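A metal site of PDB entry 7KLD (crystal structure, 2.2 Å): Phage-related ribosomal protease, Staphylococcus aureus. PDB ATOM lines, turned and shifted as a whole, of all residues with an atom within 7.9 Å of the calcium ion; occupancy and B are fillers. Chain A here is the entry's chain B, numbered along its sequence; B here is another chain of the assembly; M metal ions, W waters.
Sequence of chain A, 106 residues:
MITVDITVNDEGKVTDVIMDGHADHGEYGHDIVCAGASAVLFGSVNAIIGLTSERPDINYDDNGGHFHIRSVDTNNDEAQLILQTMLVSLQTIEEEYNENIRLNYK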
ATOM      1  N   PRO A  56      23.311 -34.476  35.668  1.00  0.00           N
ATOM      2  CA  PRO A  56      23.322 -33.033  35.465  1.00  0.00           C
ATOM      3  C   PRO A  56      23.782 -32.756  34.074  1.00  0.00           C
ATOM      4  O   PRO A  56      24.452 -33.610  33.495  1.00  0.00           O
ATOM      5  CB  PRO A  56      24.359 -32.543  36.480  1.00  0.00           C
ATOM      6  CG  PRO A  56      25.166 -33.693  36.850  1.00  0.00           C
ATOM      7  CD  PRO A  56      24.399 -34.950  36.533  1.00  0.00           C
ATOM      8  N   ASP A  57      23.428 -31.588  33.559  1.00  0.00           N
ATOM      9  CA  ASP A  57      23.921 -31.093  32.281  1.00  0.00           C
ATOM     10  C   ASP A  57      25.291 -30.450  32.491  1.00  0.00           C
ATOM     11  O   ASP A  57      25.393 -29.497  33.261  1.00  0.00           O
ATOM     12  CB  ASP A  57      22.907 -30.115  31.711  1.00  0.00           C
ATOM     13  CG  ASP A  57      23.427 -29.306  30.594  1.00  0.00           C
ATOM     14  OD1 ASP A  57      24.613 -29.543  30.179  1.00  0.00           O
ATOM     15  OD2 ASP A  57      22.632 -28.439  30.157  1.00  0.00           O
ATOM     16  N   ILE A  58      26.336 -31.006  31.850  1.00  0.00           N
ATOM     17  CA  ILE A  58      27.733 -30.691  32.146  1.00  0.00           C
ATOM     18  C   ILE A  58      28.405 -30.184  30.928  1.00  0.00           C
ATOM     19  O   ILE A  58      28.255 -30.742  29.857  1.00  0.00           O
ATOM     20  CB  ILE A  58      28.482 -31.967  32.680  1.00  0.00           C
ATOM     21  CG1 ILE A  58      27.868 -32.411  33.987  1.00  0.00           C
ATOM     22  CG2 ILE A  58      30.022 -31.795  32.849  1.00  0.00           C
ATOM     23  CD1 ILE A  58      27.675 -33.892  33.916  1.00  0.00           C
ATOM     24  N   ASN A  59      29.147 -29.079  31.064  1.00  0.00           N
ATOM     25  CA  ASN A  59      29.935 -28.515  29.971  1.00  0.00           C
ATOM     26  C   ASN A  59      31.208 -27.949  30.547  1.00  0.00           C
ATOM     27  O   ASN A  59      31.241 -27.425  31.669  1.00  0.00           O
ATOM     28  CB  ASN A  59      29.158 -27.401  29.207  1.00  0.00           C
ATOM     29  CG  ASN A  59      27.935 -27.920  28.464  1.00  0.00           C
ATOM     30  OD1 ASN A  59      26.803 -27.633  28.828  1.00  0.00           O
ATOM     31  ND2 ASN A  59      28.173 -28.664  27.408  1.00  0.00           N
ATOM     32  N   TYR A  60      32.281 -28.066  29.765  1.00  0.00           N
ATOM     33  CA  TYR A  60      33.601 -27.626  30.165  1.00  0.00           C
ATOM     34  C   TYR A  60      34.466 -27.337  28.957  1.00  0.00           C
ATOM     35  O   TYR A  60      34.158 -27.769  27.864  1.00  0.00           O
ATOM     36  CB  TYR A  60      34.268 -28.667  31.049  1.00  0.00           C
ATOM     37  CG  TYR A  60      34.599 -29.970  30.346  1.00  0.00           C
ATOM     38  CD1 TYR A  60      33.678 -31.016  30.295  1.00  0.00           C
ATOM     39  CD2 TYR A  60      35.824 -30.157  29.770  1.00  0.00           C
ATOM     40  CE1 TYR A  60      33.977 -32.186  29.640  1.00  0.00           C
ATOM     41  CE2 TYR A  60      36.148 -31.336  29.134  1.00  0.00           C
ATOM     42  CZ  TYR A  60      35.217 -32.355  29.087  1.00  0.00           C
ATOM     43  OH  TYR A  60      35.537 -33.536  28.461  1.00  0.00           O
ATOM     44  N   HIS A  68      31.050 -26.102  33.994  1.00  0.00           N
ATOM     45  CA  HIS A  68      29.720 -25.709  34.266  1.00  0.00           C
ATOM     46  C   HIS A  68      28.841 -26.911  34.597  1.00  0.00           C
ATOM     47  O   HIS A  68      28.741 -27.830  33.804  1.00  0.00           O
ATOM     48  CB  HIS A  68      29.177 -25.118  32.998  1.00  0.00           C
ATOM     49  CG  HIS A  68      27.747 -24.711  33.060  1.00  0.00           C
ATOM     50  ND1 HIS A  68      26.923 -24.794  31.978  1.00  0.00           N
ATOM     51  CD2 HIS A  68      27.000 -24.206  34.056  1.00  0.00           C
ATOM     52  CE1 HIS A  68      25.733 -24.340  32.296  1.00  0.00           C
ATOM     53  NE2 HIS A  68      25.751 -23.984  33.555  1.00  0.00           N
ATOM     54  N   ILE A  69      28.199 -26.890  35.757  1.00  0.00           N
ATOM     55  CA  ILE A  69      27.260 -27.901  36.140  1.00  0.00           C
ATOM     56  C   ILE A  69      25.868 -27.286  36.281  1.00  0.00           C
ATOM     57  O   ILE A  69      25.697 -26.284  36.898  1.00  0.00           O
ATOM     58  CB  ILE A  69      27.589 -28.519  37.532  1.00  0.00           C
ATOM     59  CG1 ILE A  69      28.990 -28.992  37.653  1.00  0.00           C
ATOM     60  CG2 ILE A  69      26.704 -29.694  37.811  1.00  0.00           C
ATOM     61  CD1 ILE A  69      29.443 -29.004  39.064  1.00  0.00           C
ATOM     62  N   ARG A  70      24.867 -27.901  35.688  1.00  0.00           N
ATOM     63  CA  ARG A  70      23.524 -27.428  35.831  1.00  0.00           C
ATOM     64  C   ARG A  70      22.634 -28.579  36.262  1.00  0.00           C
ATOM     65  O   ARG A  70      22.623 -29.615  35.633  1.00  0.00           O
ATOM     66  CB  ARG A  70      22.970 -26.795  34.559  1.00  0.00           C
ATOM     67  CG  ARG A  70      21.632 -26.141  34.792  1.00  0.00           C
ATOM     68  CD  ARG A  70      21.211 -25.318  33.601  1.00  0.00           C
ATOM     69  NE  ARG A  70      21.852 -24.022  33.680  1.00  0.00           N
ATOM     70  CZ  ARG A  70      22.052 -23.195  32.688  1.00  0.00           C
ATOM     71  NH1 ARG A  70      21.675 -23.498  31.466  1.00  0.00           N
ATOM     72  NH2 ARG A  70      22.633 -22.049  32.934  1.00  0.00           N
ATOM     73  N   MET B  19      25.458 -18.786  27.367  1.00  0.00           N
ATOM     74  CA  MET B  19      24.501 -19.374  26.461  1.00  0.00           C
ATOM     75  C   MET B  19      24.673 -20.872  26.491  1.00  0.00           C
ATOM     76  O   MET B  19      25.757 -21.380  26.233  1.00  0.00           O
ATOM     77  CB  MET B  19      24.706 -18.853  25.039  1.00  0.00           C
ATOM     78  CG  MET B  19      24.335 -17.388  24.934  1.00  0.00           C
ATOM     79  SD  MET B  19      24.953 -16.587  23.405  1.00  0.00           S
ATOM     80  CE  MET B  19      23.728 -17.226  22.252  1.00  0.00           C
ATOM     81  N   ASP B  20      23.582 -21.593  26.733  1.00  0.00           N
ATOM     82  CA  ASP B  20      23.710 -23.030  26.875  1.00  0.00           C
ATOM     83  C   ASP B  20      22.440 -23.723  26.456  1.00  0.00           C
ATOM     84  O   ASP B  20      21.346 -23.249  26.722  1.00  0.00           O
ATOM     85  CB  ASP B  20      24.104 -23.380  28.319  1.00  0.00           C
ATOM     86  CG  ASP B  20      24.582 -24.786  28.455  1.00  0.00           C
ATOM     87  OD1 ASP B  20      23.717 -25.659  28.685  1.00  0.00           O
ATOM     88  OD2 ASP B  20      25.810 -25.027  28.352  1.00  0.00           O
ATOM     89  N   GLY B  21      22.638 -24.909  25.876  1.00  0.00           N
ATOM     90  CA  GLY B  21      21.598 -25.684  25.229  1.00  0.00           C
ATOM     91  C   GLY B  21      21.482 -25.491  23.738  1.00  0.00           C
ATOM     92  O   GLY B  21      22.134 -24.611  23.143  1.00  0.00           O
ATOM     93  N   HIS B  22      20.620 -26.306  23.136  1.00  0.00           N
ATOM     94  CA  HIS B  22      20.308 -26.172  21.721  1.00  0.00           C
ATOM     95  C   HIS B  22      18.846 -25.795  21.579  1.00  0.00           C
ATOM     96  O   HIS B  22      17.991 -26.264  22.341  1.00  0.00           O
ATOM     97  CB  HIS B  22      20.635 -27.474  20.994  1.00  0.00           C
ATOM     98  CG  HIS B  22      22.080 -27.859  21.092  1.00  0.00           C
ATOM     99  ND1 HIS B  22      22.626 -28.425  22.233  1.00  0.00           N
ATOM    100  CD2 HIS B  22      23.096 -27.777  20.196  1.00  0.00           C
ATOM    101  CE1 HIS B  22      23.914 -28.646  22.038  1.00  0.00           C
ATOM    102  NE2 HIS B  22      24.221 -28.265  20.813  1.00  0.00           N
ATOM    103  N   ASP B  61      32.574 -24.982  24.946  1.00  0.00           N
ATOM    104  CA  ASP B  61      32.740 -26.376  24.868  1.00  0.00           C
ATOM    105  C   ASP B  61      32.927 -26.686  23.431  1.00  0.00           C
ATOM    106  O   ASP B  61      32.175 -26.222  22.655  1.00  0.00           O
ATOM    107  CB  ASP B  61      31.461 -27.027  25.376  1.00  0.00           C
ATOM    108  CG  ASP B  61      31.583 -28.501  25.550  1.00  0.00           C
ATOM    109  OD1 ASP B  61      31.365 -29.021  26.637  1.00  0.00           O
ATOM    110  OD2 ASP B  61      31.849 -29.171  24.585  1.00  0.00           O
ATOM    111  N   GLY B  64      29.689 -27.762  21.309  1.00  0.00           N
ATOM    112  CA  GLY B  64      28.489 -27.016  21.109  1.00  0.00           C
ATOM    113  C   GLY B  64      27.568 -26.906  22.308  1.00  0.00           C
ATOM    114  O   GLY B  64      27.669 -27.628  23.284  1.00  0.00           O
ATOM    115  N   GLY B  65      26.543 -26.008  22.254  1.00  0.00           N
ATOM    116  CA  GLY B  65      25.614 -25.743  23.291  1.00  0.00           C
ATOM    117  C   GLY B  65      26.224 -25.090  24.470  1.00  0.00           C
ATOM    118  O   GLY B  65      25.624 -25.206  25.461  1.00  0.00           O
ATOM    119  N   HIS B  66      27.403 -24.459  24.410  1.00  0.00           N
ATOM    120  CA  HIS B  66      27.963 -23.860  25.574  1.00  0.00           C
ATOM    121  C   HIS B  66      29.003 -22.816  25.279  1.00  0.00           C
ATOM    122  O   HIS B  66      29.985 -23.141  24.782  1.00  0.00           O
ATOM    123  CB  HIS B  66      28.642 -24.836  26.460  1.00  0.00           C
ATOM    124  CG  HIS B  66      29.005 -24.284  27.771  1.00  0.00           C
ATOM    125  ND1 HIS B  66      28.081 -23.755  28.605  1.00  0.00           N
ATOM    126  CD2 HIS B  66      30.169 -24.169  28.414  1.00  0.00           C
ATOM    127  CE1 HIS B  66      28.637 -23.362  29.706  1.00  0.00           C
ATOM    128  NE2 HIS B  66      29.907 -23.556  29.590  1.00  0.00           N
HETATM  129 CA    CA M   1      24.804 -27.856  28.632  1.00  0.00          CA
HETATM  130  O   HOH W   1      24.179 -27.505  26.655  1.00  0.00           O
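Water W1 lies within hydrogen-bond range of O of Gly 65 of chain B (3.0 Å), N of Gly 21 of chain B (3.1 Å) and OD2 of Asp 20 of chain B (3.4 Å).
Of the 16 residues printed, 3 come within 4 Å of the calcium ion.
The backbone carbonyl oxygen (O) of Asn 59 sits at hydrogen-bond distance from the backbone NH (N) of His 68, 2.7 Å away.
O of Asp 57 lies within hydrogen-bond range of N of Arg 70, at 3.0 Å.
The side-chain amide nitrogen of Asn 59 is in hydrogen-bond range of the side-chain carboxylate of Asp 61 of chain B.
The side-chain carboxylate of Asp 20 of chain B is in hydrogen-bond range of a ring nitrogen (ND1) of His 66 of chain B.
The side-chain amide oxygen (OD1) of Asn 59 binds the calcium ion, at 2.0 Å.
Water W1 binds the calcium ion, 2.1 Å away.
OD1 of Asp 57 is bound to the calcium ion (2.3 Å).
The side-chain carboxylate (OD1) of Asp 20 of chain B binds the calcium ion (2.5 Å).
The calcium ion is bound by OD2 of Asp 57 (2.7 Å).
Slightly farther from the calcium ion lies the side-chain carboxylate (OD2) of Asp 20 of chain B (3.0 Å).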
